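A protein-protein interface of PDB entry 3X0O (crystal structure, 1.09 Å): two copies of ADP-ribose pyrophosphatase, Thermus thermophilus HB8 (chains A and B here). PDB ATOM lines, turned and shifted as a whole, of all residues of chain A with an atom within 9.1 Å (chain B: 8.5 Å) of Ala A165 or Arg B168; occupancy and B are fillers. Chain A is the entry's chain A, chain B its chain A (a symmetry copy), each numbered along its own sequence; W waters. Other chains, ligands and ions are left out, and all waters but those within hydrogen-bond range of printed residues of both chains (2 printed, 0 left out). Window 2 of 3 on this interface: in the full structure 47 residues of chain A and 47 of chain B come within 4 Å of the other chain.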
ATOM      1  N   MET A  47     -24.085   7.348 -38.127  1.00  0.00           N
ATOM      2  CA  MET A  47     -23.820   8.638 -37.504  1.00  0.00           C
ATOM      3  C   MET A  47     -23.018   9.496 -38.460  1.00  0.00           C
ATOM      4  O   MET A  47     -22.185   9.035 -39.253  1.00  0.00           O
ATOM      5  CB  MET A  47     -23.062   8.395 -36.192  1.00  0.00           C
ATOM      6  CG  MET A  47     -22.594   9.667 -35.488  1.00  0.00           C
ATOM      7  SD  MET A  47     -22.290   9.321 -33.695  1.00  0.00           S
ATOM      8  CE  MET A  47     -23.869   8.937 -33.144  1.00  0.00           C
ATOM      9  N   PHE A  97     -26.069  18.329 -23.484  1.00  0.00           N
ATOM     10  CA  PHE A  97     -25.176  18.475 -22.329  1.00  0.00           C
ATOM     11  C   PHE A  97     -23.911  19.199 -22.792  1.00  0.00           C
ATOM     12  O   PHE A  97     -23.730  19.443 -24.006  1.00  0.00           O
ATOM     13  CB  PHE A  97     -24.831  17.120 -21.685  1.00  0.00           C
ATOM     14  CG  PHE A  97     -24.583  15.969 -22.655  1.00  0.00           C
ATOM     15  CD1 PHE A  97     -25.389  14.831 -22.549  1.00  0.00           C
ATOM     16  CD2 PHE A  97     -23.544  16.018 -23.614  1.00  0.00           C
ATOM     17  CE1 PHE A  97     -25.170  13.770 -23.412  1.00  0.00           C
ATOM     18  CE2 PHE A  97     -23.362  14.989 -24.511  1.00  0.00           C
ATOM     19  CZ  PHE A  97     -24.223  13.849 -24.437  1.00  0.00           C
ATOM     20  N   PRO A 138     -22.173   3.786 -35.881  1.00  0.00           N
ATOM     21  CA  PRO A 138     -21.319   3.962 -34.722  1.00  0.00           C
ATOM     22  C   PRO A 138     -20.653   2.651 -34.241  1.00  0.00           C
ATOM     23  O   PRO A 138     -19.571   2.721 -33.647  1.00  0.00           O
ATOM     24  CB  PRO A 138     -22.266   4.468 -33.617  1.00  0.00           C
ATOM     25  CG  PRO A 138     -23.369   5.095 -34.396  1.00  0.00           C
ATOM     26  CD  PRO A 138     -23.519   4.302 -35.664  1.00  0.00           C
ATOM     27  N   LEU A 157     -15.990  10.429 -29.890  1.00  0.00           N
ATOM     28  CA  LEU A 157     -16.224   9.416 -28.880  1.00  0.00           C
ATOM     29  C   LEU A 157     -17.517   9.662 -28.143  1.00  0.00           C
ATOM     30  O   LEU A 157     -18.302   8.726 -27.896  1.00  0.00           O
ATOM     31  CB  LEU A 157     -15.034   9.379 -27.906  1.00  0.00           C
ATOM     32  CG  LEU A 157     -15.201   8.393 -26.755  1.00  0.00           C
ATOM     33  CD1 LEU A 157     -15.331   6.943 -27.240  1.00  0.00           C
ATOM     34  CD2 LEU A 157     -14.003   8.558 -25.811  1.00  0.00           C
ATOM     35  N   VAL A 158     -17.778  10.908 -27.785  1.00  0.00           N
ATOM     36  CA  VAL A 158     -19.062  11.252 -27.105  1.00  0.00           C
ATOM     37  C   VAL A 158     -20.231  10.867 -28.001  1.00  0.00           C
ATOM     38  O   VAL A 158     -21.218  10.306 -27.515  1.00  0.00           O
ATOM     39  CB  VAL A 158     -19.046  12.741 -26.737  1.00  0.00           C
ATOM     40  CG1 VAL A 158     -20.463  13.260 -26.431  1.00  0.00           C
ATOM     41  CG2 VAL A 158     -18.089  12.977 -25.548  1.00  0.00           C
ATOM     42  N   GLY A 159     -20.138  11.158 -29.328  1.00  0.00           N
ATOM     43  CA  GLY A 159     -21.250  10.765 -30.201  1.00  0.00           C
ATOM     44  C   GLY A 159     -21.468   9.255 -30.189  1.00  0.00           C
ATOM     45  O   GLY A 159     -22.586   8.751 -30.102  1.00  0.00           O
ATOM     46  N   VAL A 160     -20.371   8.483 -30.306  1.00  0.00           N
ATOM     47  CA  VAL A 160     -20.503   7.019 -30.342  1.00  0.00           C
ATOM     48  C   VAL A 160     -21.084   6.496 -29.028  1.00  0.00           C
ATOM     49  O   VAL A 160     -21.936   5.602 -29.031  1.00  0.00           O
ATOM     50  CB  VAL A 160     -19.116   6.404 -30.634  1.00  0.00           C
ATOM     51  CG1 VAL A 160     -19.070   4.908 -30.347  1.00  0.00           C
ATOM     52  CG2 VAL A 160     -18.710   6.706 -32.086  1.00  0.00           C
ATOM     53  N   LEU A 161     -20.597   7.018 -27.889  1.00  0.00           N
ATOM     54  CA  LEU A 161     -21.101   6.507 -26.621  1.00  0.00           C
ATOM     55  C   LEU A 161     -22.541   6.942 -26.384  1.00  0.00           C
ATOM     56  O   LEU A 161     -23.344   6.133 -25.902  1.00  0.00           O
ATOM     57  CB  LEU A 161     -20.217   7.005 -25.441  1.00  0.00           C
ATOM     58  CG  LEU A 161     -18.786   6.460 -25.500  1.00  0.00           C
ATOM     59  CD1 LEU A 161     -17.964   7.035 -24.321  1.00  0.00           C
ATOM     60  CD2 LEU A 161     -18.733   4.926 -25.453  1.00  0.00           C
ATOM     61  N   TYR A 162     -22.884   8.184 -26.753  1.00  0.00           N
ATOM     62  CA  TYR A 162     -24.275   8.597 -26.597  1.00  0.00           C
ATOM     63  C   TYR A 162     -25.197   7.708 -27.433  1.00  0.00           C
ATOM     64  O   TYR A 162     -26.282   7.339 -26.948  1.00  0.00           O
ATOM     65  CB  TYR A 162     -24.383  10.066 -27.086  1.00  0.00           C
ATOM     66  CG  TYR A 162     -25.821  10.566 -26.854  1.00  0.00           C
ATOM     67  CD1 TYR A 162     -26.203  11.045 -25.599  1.00  0.00           C
ATOM     68  CD2 TYR A 162     -26.756  10.525 -27.882  1.00  0.00           C
ATOM     69  CE1 TYR A 162     -27.502  11.502 -25.385  1.00  0.00           C
ATOM     70  CE2 TYR A 162     -28.067  10.944 -27.667  1.00  0.00           C
ATOM     71  CZ  TYR A 162     -28.413  11.430 -26.436  1.00  0.00           C
ATOM     72  OH  TYR A 162     -29.733  11.829 -26.247  1.00  0.00           O
ATOM     73  N   TYR A 163     -24.812   7.398 -28.661  1.00  0.00           N
ATOM     74  CA  TYR A 163     -25.658   6.523 -29.471  1.00  0.00           C
ATOM     75  C   TYR A 163     -25.871   5.206 -28.748  1.00  0.00           C
ATOM     76  O   TYR A 163     -26.978   4.687 -28.703  1.00  0.00           O
ATOM     77  CB  TYR A 163     -24.967   6.312 -30.846  1.00  0.00           C
ATOM     78  CG  TYR A 163     -25.484   5.049 -31.559  1.00  0.00           C
ATOM     79  CD1 TYR A 163     -26.641   5.186 -32.355  1.00  0.00           C
ATOM     80  CD2 TYR A 163     -24.861   3.814 -31.462  1.00  0.00           C
ATOM     81  CE1 TYR A 163     -27.104   4.040 -33.007  1.00  0.00           C
ATOM     82  CE2 TYR A 163     -25.315   2.663 -32.107  1.00  0.00           C
ATOM     83  CZ  TYR A 163     -26.445   2.803 -32.871  1.00  0.00           C
ATOM     84  OH  TYR A 163     -26.943   1.665 -33.543  1.00  0.00           O
ATOM     85  N   HIS A 164     -24.771   4.574 -28.289  1.00  0.00           N
ATOM     86  CA  HIS A 164     -24.941   3.235 -27.711  1.00  0.00           C
ATOM     87  C   HIS A 164     -25.785   3.304 -26.416  1.00  0.00           C
ATOM     88  O   HIS A 164     -26.449   2.336 -26.115  1.00  0.00           O
ATOM     89  CB  HIS A 164     -23.549   2.657 -27.412  1.00  0.00           C
ATOM     90  CG  HIS A 164     -22.852   2.098 -28.596  1.00  0.00           C
ATOM     91  ND1 HIS A 164     -22.058   2.843 -29.424  1.00  0.00           N
ATOM     92  CD2 HIS A 164     -22.840   0.801 -29.076  1.00  0.00           C
ATOM     93  CE1 HIS A 164     -21.573   2.034 -30.376  1.00  0.00           C
ATOM     94  NE2 HIS A 164     -22.027   0.793 -30.191  1.00  0.00           N
ATOM     95  N   ALA A 165     -25.706   4.421 -25.686  1.00  0.00           N
ATOM     96  CA  ALA A 165     -26.475   4.554 -24.457  1.00  0.00           C
ATOM     97  C   ALA A 165     -27.955   4.782 -24.729  1.00  0.00           C
ATOM     98  O   ALA A 165     -28.810   4.242 -24.018  1.00  0.00           O
ATOM     99  CB  ALA A 165     -25.929   5.737 -23.662  1.00  0.00           C
ATOM    100  N   PHE A 166     -28.267   5.633 -25.741  1.00  0.00           N
ATOM    101  CA  PHE A 166     -29.629   6.172 -25.790  1.00  0.00           C
ATOM    102  C   PHE A 166     -30.293   6.093 -27.135  1.00  0.00           C
ATOM    103  O   PHE A 166     -31.526   6.382 -27.175  1.00  0.00           O
ATOM    104  CB  PHE A 166     -29.640   7.678 -25.342  1.00  0.00           C
ATOM    105  CG  PHE A 166     -29.092   7.916 -23.955  1.00  0.00           C
ATOM    106  CD1 PHE A 166     -27.956   8.663 -23.708  1.00  0.00           C
ATOM    107  CD2 PHE A 166     -29.754   7.367 -22.844  1.00  0.00           C
ATOM    108  CE1 PHE A 166     -27.467   8.865 -22.439  1.00  0.00           C
ATOM    109  CE2 PHE A 166     -29.248   7.533 -21.534  1.00  0.00           C
ATOM    110  CZ  PHE A 166     -28.121   8.285 -21.342  1.00  0.00           C
ATOM    111  N   LEU A 167     -29.606   5.739 -28.230  1.00  0.00           N
ATOM    112  CA  LEU A 167     -30.263   5.838 -29.518  1.00  0.00           C
ATOM    113  C   LEU A 167     -30.491   4.493 -30.206  1.00  0.00           C
ATOM    114  O   LEU A 167     -30.888   4.509 -31.397  1.00  0.00           O
ATOM    115  CB  LEU A 167     -29.444   6.770 -30.428  1.00  0.00           C
ATOM    116  CG  LEU A 167     -29.262   8.202 -29.973  1.00  0.00           C
ATOM    117  CD1 LEU A 167     -28.394   8.949 -31.000  1.00  0.00           C
ATOM    118  CD2 LEU A 167     -30.587   8.926 -29.773  1.00  0.00           C
ATOM    119  N   ARG A 168     -30.306   3.363 -29.571  1.00  0.00           N
ATOM    120  CA  ARG A 168     -30.544   2.059 -30.224  1.00  0.00           C
ATOM    121  C   ARG A 168     -31.931   1.454 -30.061  1.00  0.00           C
ATOM    122  O   ARG A 168     -32.830   2.225 -29.778  1.00  0.00           O
ATOM    123  CB  ARG A 168     -29.559   1.019 -29.669  1.00  0.00           C
ATOM    124  CG  ARG A 168     -28.129   1.486 -30.001  1.00  0.00           C
ATOM    125  CD  ARG A 168     -27.185   0.315 -29.808  1.00  0.00           C
ATOM    126  NE  ARG A 168     -26.959   0.252 -28.343  1.00  0.00           N
ATOM    127  CZ  ARG A 168     -26.207  -0.696 -27.795  1.00  0.00           C
ATOM    128  NH1 ARG A 168     -25.700  -1.587 -28.651  1.00  0.00           N
ATOM    129  NH2 ARG A 168     -26.033  -0.705 -26.484  1.00  0.00           N
ATOM    130  N   LEU B  42     -16.946   1.396 -11.237  1.00  0.00           N
ATOM    131  CA  LEU B  42     -18.322   1.263 -10.772  1.00  0.00           C
ATOM    132  C   LEU B  42     -18.240   0.368  -9.514  1.00  0.00           C
ATOM    133  O   LEU B  42     -17.586  -0.671  -9.521  1.00  0.00           O
ATOM    134  CB  LEU B  42     -19.209   0.700 -11.883  1.00  0.00           C
ATOM    135  CG  LEU B  42     -20.718   0.858 -11.714  1.00  0.00           C
ATOM    136  CD1 LEU B  42     -21.123   2.310 -11.932  1.00  0.00           C
ATOM    137  CD2 LEU B  42     -21.456  -0.067 -12.671  1.00  0.00           C
ATOM    138  N   ARG B 137     -24.171   7.682  -8.187  1.00  0.00           N
ATOM    139  CA  ARG B 137     -24.793   6.971  -9.317  1.00  0.00           C
ATOM    140  C   ARG B 137     -24.682   7.760 -10.607  1.00  0.00           C
ATOM    141  O   ARG B 137     -24.951   8.957 -10.600  1.00  0.00           O
ATOM    142  CB  ARG B 137     -26.288   6.727  -9.006  1.00  0.00           C
ATOM    143  CG  ARG B 137     -26.430   5.822  -7.754  1.00  0.00           C
ATOM    144  CD  ARG B 137     -27.917   5.665  -7.372  1.00  0.00           C
ATOM    145  NE  ARG B 137     -28.801   5.394  -8.471  1.00  0.00           N
ATOM    146  CZ  ARG B 137     -29.645   5.986  -9.312  1.00  0.00           C
ATOM    147  NH1 ARG B 137     -30.312   5.283 -10.251  1.00  0.00           N
ATOM    148  NH2 ARG B 137     -29.894   7.314  -9.300  1.00  0.00           N
ATOM    149  N   PRO B 138     -24.258   7.156 -11.711  1.00  0.00           N
ATOM    150  CA  PRO B 138     -24.150   7.947 -12.922  1.00  0.00           C
ATOM    151  C   PRO B 138     -25.489   8.581 -13.366  1.00  0.00           C
ATOM    152  O   PRO B 138     -25.458   9.630 -14.020  1.00  0.00           O
ATOM    153  CB  PRO B 138     -23.697   6.944 -14.000  1.00  0.00           C
ATOM    154  CG  PRO B 138     -23.021   5.888 -13.198  1.00  0.00           C
ATOM    155  CD  PRO B 138     -23.744   5.803 -11.884  1.00  0.00           C
ATOM    156  N   GLU B 139     -26.603   7.935 -13.084  1.00  0.00           N
ATOM    157  CA  GLU B 139     -27.913   8.499 -13.398  1.00  0.00           C
ATOM    158  C   GLU B 139     -28.083   9.822 -12.664  1.00  0.00           C
ATOM    159  O   GLU B 139     -28.622  10.747 -13.272  1.00  0.00           O
ATOM    160  CB  GLU B 139     -28.956   7.485 -12.908  1.00  0.00           C
ATOM    161  CG  GLU B 139     -28.981   6.176 -13.674  1.00  0.00           C
ATOM    162  CD  GLU B 139     -28.146   5.052 -13.119  1.00  0.00           C
ATOM    163  OE1 GLU B 139     -27.270   5.351 -12.247  1.00  0.00           O
ATOM    164  OE2 GLU B 139     -28.314   3.894 -13.556  1.00  0.00           O
ATOM    165  N   LEU B 142     -25.830  12.542 -14.190  1.00  0.00           N
ATOM    166  CA  LEU B 142     -26.430  13.101 -15.418  1.00  0.00           C
ATOM    167  C   LEU B 142     -27.572  14.009 -15.046  1.00  0.00           C
ATOM    168  O   LEU B 142     -27.697  15.130 -15.597  1.00  0.00           O
ATOM    169  CB  LEU B 142     -26.877  11.914 -16.299  1.00  0.00           C
ATOM    170  CG  LEU B 142     -27.492  12.350 -17.671  1.00  0.00           C
ATOM    171  CD1 LEU B 142     -26.581  13.296 -18.415  1.00  0.00           C
ATOM    172  CD2 LEU B 142     -27.767  11.077 -18.474  1.00  0.00           C
ATOM    173  N   VAL B 160     -19.878   8.673 -17.619  1.00  0.00           N
ATOM    174  CA  VAL B 160     -21.338   8.538 -17.498  1.00  0.00           C
ATOM    175  C   VAL B 160     -21.926   7.885 -18.748  1.00  0.00           C
ATOM    176  O   VAL B 160     -22.812   7.030 -18.651  1.00  0.00           O
ATOM    177  CB  VAL B 160     -21.946   9.937 -17.248  1.00  0.00           C
ATOM    178  CG1 VAL B 160     -23.454   9.961 -17.456  1.00  0.00           C
ATOM    179  CG2 VAL B 160     -21.568  10.421 -15.838  1.00  0.00           C
ATOM    180  N   LEU B 161     -21.469   8.312 -19.938  1.00  0.00           N
ATOM    181  CA  LEU B 161     -22.044   7.739 -21.148  1.00  0.00           C
ATOM    182  C   LEU B 161     -21.612   6.289 -21.331  1.00  0.00           C
ATOM    183  O   LEU B 161     -22.441   5.458 -21.725  1.00  0.00           O
ATOM    184  CB  LEU B 161     -21.616   8.559 -22.399  1.00  0.00           C
ATOM    185  CG  LEU B 161     -22.167   9.989 -22.387  1.00  0.00           C
ATOM    186  CD1 LEU B 161     -21.661  10.749 -23.638  1.00  0.00           C
ATOM    187  CD2 LEU B 161     -23.702  10.034 -22.354  1.00  0.00           C
ATOM    188  N   TYR B 162     -20.350   5.972 -21.012  1.00  0.00           N
ATOM    189  CA  TYR B 162     -19.936   4.576 -21.114  1.00  0.00           C
ATOM    190  C   TYR B 162     -20.773   3.697 -20.184  1.00  0.00           C
ATOM    191  O   TYR B 162     -21.161   2.585 -20.590  1.00  0.00           O
ATOM    192  CB  TYR B 162     -18.443   4.501 -20.701  1.00  0.00           C
ATOM    193  CG  TYR B 162     -17.946   3.054 -20.881  1.00  0.00           C
ATOM    194  CD1 TYR B 162     -17.532   2.607 -22.138  1.00  0.00           C
ATOM    195  CD2 TYR B 162     -17.925   2.175 -19.804  1.00  0.00           C
ATOM    196  CE1 TYR B 162     -17.079   1.300 -22.307  1.00  0.00           C
ATOM    197  CE2 TYR B 162     -17.510   0.857 -19.971  1.00  0.00           C
ATOM    198  CZ  TYR B 162     -17.088   0.447 -21.206  1.00  0.00           C
ATOM    199  OH  TYR B 162     -16.691  -0.879 -21.345  1.00  0.00           O
ATOM    200  N   TYR B 163     -21.019   4.146 -18.963  1.00  0.00           N
ATOM    201  CA  TYR B 163     -21.844   3.341 -18.064  1.00  0.00           C
ATOM    202  C   TYR B 163     -23.197   3.084 -18.702  1.00  0.00           C
ATOM    203  O   TYR B 163     -23.710   1.975 -18.660  1.00  0.00           O
ATOM    204  CB  TYR B 163     -21.985   4.105 -16.718  1.00  0.00           C
ATOM    205  CG  TYR B 163     -23.206   3.622 -15.911  1.00  0.00           C
ATOM    206  CD1 TYR B 163     -23.017   2.510 -15.063  1.00  0.00           C
ATOM    207  CD2 TYR B 163     -24.448   4.233 -15.975  1.00  0.00           C
ATOM    208  CE1 TYR B 163     -24.124   2.078 -14.327  1.00  0.00           C
ATOM    209  CE2 TYR B 163     -25.560   3.811 -15.245  1.00  0.00           C
ATOM    210  CZ  TYR B 163     -25.371   2.724 -14.430  1.00  0.00           C
ATOM    211  OH  TYR B 163     -26.468   2.259 -13.673  1.00  0.00           O
ATOM    212  N   HIS B 164     -23.859   4.156 -19.185  1.00  0.00           N
ATOM    213  CA  HIS B 164     -25.227   3.950 -19.679  1.00  0.00           C
ATOM    214  C   HIS B 164     -25.222   3.037 -20.929  1.00  0.00           C
ATOM    215  O   HIS B 164     -26.199   2.354 -21.142  1.00  0.00           O
ATOM    216  CB  HIS B 164     -25.829   5.321 -20.021  1.00  0.00           C
ATOM    217  CG  HIS B 164     -26.329   6.079 -18.848  1.00  0.00           C
ATOM    218  ND1 HIS B 164     -25.546   6.920 -18.105  1.00  0.00           N
ATOM    219  CD2 HIS B 164     -27.598   6.112 -18.300  1.00  0.00           C
ATOM    220  CE1 HIS B 164     -26.306   7.452 -17.138  1.00  0.00           C
ATOM    221  NE2 HIS B 164     -27.552   6.984 -17.231  1.00  0.00           N
ATOM    222  N   ALA B 165     -24.146   3.082 -21.721  1.00  0.00           N
ATOM    223  CA  ALA B 165     -24.073   2.248 -22.913  1.00  0.00           C
ATOM    224  C   ALA B 165     -23.821   0.786 -22.575  1.00  0.00           C
ATOM    225  O   ALA B 165     -24.392  -0.109 -23.209  1.00  0.00           O
ATOM    226  CB  ALA B 165     -22.939   2.755 -23.799  1.00  0.00           C
ATOM    227  N   PHE B 166     -22.915   0.531 -21.595  1.00  0.00           N
ATOM    228  CA  PHE B 166     -22.365  -0.822 -21.502  1.00  0.00           C
ATOM    229  C   PHE B 166     -22.367  -1.414 -20.121  1.00  0.00           C
ATOM    230  O   PHE B 166     -22.068  -2.642 -20.031  1.00  0.00           O
ATOM    231  CB  PHE B 166     -20.884  -0.852 -22.029  1.00  0.00           C
ATOM    232  CG  PHE B 166     -20.725  -0.379 -23.454  1.00  0.00           C
ATOM    233  CD1 PHE B 166     -20.000   0.745 -23.802  1.00  0.00           C
ATOM    234  CD2 PHE B 166     -21.328  -1.102 -24.497  1.00  0.00           C
ATOM    235  CE1 PHE B 166     -19.869   1.166 -25.104  1.00  0.00           C
ATOM    236  CE2 PHE B 166     -21.237  -0.667 -25.840  1.00  0.00           C
ATOM    237  CZ  PHE B 166     -20.503   0.452 -26.132  1.00  0.00           C
ATOM    238  N   LEU B 167     -22.667  -0.671 -19.047  1.00  0.00           N
ATOM    239  CA  LEU B 167     -22.494  -1.257 -17.733  1.00  0.00           C
ATOM    240  C   LEU B 167     -23.799  -1.453 -16.962  1.00  0.00           C
ATOM    241  O   LEU B 167     -23.716  -1.785 -15.754  1.00  0.00           O
ATOM    242  CB  LEU B 167     -21.520  -0.386 -16.920  1.00  0.00           C
ATOM    243  CG  LEU B 167     -20.116  -0.224 -17.460  1.00  0.00           C
ATOM    244  CD1 LEU B 167     -19.321   0.701 -16.522  1.00  0.00           C
ATOM    245  CD2 LEU B 167     -19.394  -1.555 -17.628  1.00  0.00           C
ATOM    246  N   ARG B 168     -24.962  -1.307 -17.545  1.00  0.00           N
ATOM    247  CA  ARG B 168     -26.228  -1.514 -16.810  1.00  0.00           C
ATOM    248  C   ARG B 168     -26.832  -2.911 -16.866  1.00  0.00           C
ATOM    249  O   ARG B 168     -26.070  -3.821 -17.142  1.00  0.00           O
ATOM    250  CB  ARG B 168     -27.303  -0.565 -17.360  1.00  0.00           C
ATOM    251  CG  ARG B 168     -26.829   0.883 -17.132  1.00  0.00           C
ATOM    252  CD  ARG B 168     -28.014   1.810 -17.311  1.00  0.00           C
ATOM    253  NE  ARG B 168     -28.157   1.957 -18.781  1.00  0.00           N
ATOM    254  CZ  ARG B 168     -29.138   2.675 -19.316  1.00  0.00           C
ATOM    255  NH1 ARG B 168     -29.986   3.224 -18.442  1.00  0.00           N
ATOM    256  NH2 ARG B 168     -29.219   2.778 -20.632  1.00  0.00           N
HETATM  257  O   HOH W   1     -31.412   3.968 -22.153  1.00  0.00           O
HETATM  258  O   HOH W   2     -24.748  -2.808 -24.915  1.00  0.00           O
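O of His B164 sits at hydrogen-bond distance from NH2 of Arg B168 (3.1 Å).
O of His A164 sits at hydrogen-bond distance from NH2 of Arg A168.
O of Val B160 sits at hydrogen-bond distance from ND1 of His B164, 2.8 Å away.
O of Val A160 sits at hydrogen-bond distance from ND1 of His A164 (2.8 Å).
Val A158 touches Leu B161.
Leu A161 touches Leu B161.
CB of Ala B165 touches O of Leu A161, 3.9997 Å away.
Ala B165 touches His A164 (CB to CB, 3.7 Å).
His B164 touches Ala A165.
Ala A165 touches Ala B165.
Ala A165 touches Arg B168.
Leu B161 touches Phe A166.
Phe A166 touches His B164.
NH2 of Arg A168 touches O of Ala B165, at 3.7 Å.
Of the printed residues of chain B, His A164 touches Ala B165 (3.7 Å) and Phe B166 (3.8 Å).
Printed residues of chain B within 4 Å of Ala A165: Leu B161 (3.999 Å), His B164 (3.7 Å), Ala B165 (3.7 Å) and Arg B168 (3.7 Å).
Leu A167 touches none of the printed residues of chain B.
Of the printed residues of chain B, Arg A168 touches Ala B165.
Of the printed residues of chain A, Leu B161 touches Val A158, Leu A161, Ala A165 and Phe A166.
Arg B168 touches just one residue of chain A: Ala A165 (3.7 Å).
The nearest residue of chain A that does not touch Arg B168 is Phe A166 (4.8 Å).
The nearest printed residue of chain B that does not touch His A164 is His B164 (5.0 Å).
Hydrophobic or aromatic side chains of chain B that line the printed part of chain A: Leu B161, His B164, Ala B165 and Phe B166.
Leu A161 touches its own counterpart, Leu B161.
Leu A161 touches Phe B166, and with the chains exchanged Phe A166 touches Leu B161.
His A164 touches Ala B165, and with the chains exchanged Ala A165 touches His B164.
Ala B165 touches its own counterpart, Ala A165.
Water W1 lies within hydrogen-bond range of the guanidinium group of Arg B168 (2.9 Å) and the backbone carbonyl oxygen of Ala A165 (3.2 Å).
Water W2 bridges NH2 of Arg A168 (2.9 Å) and O of Ala B165 (3.2 Å).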
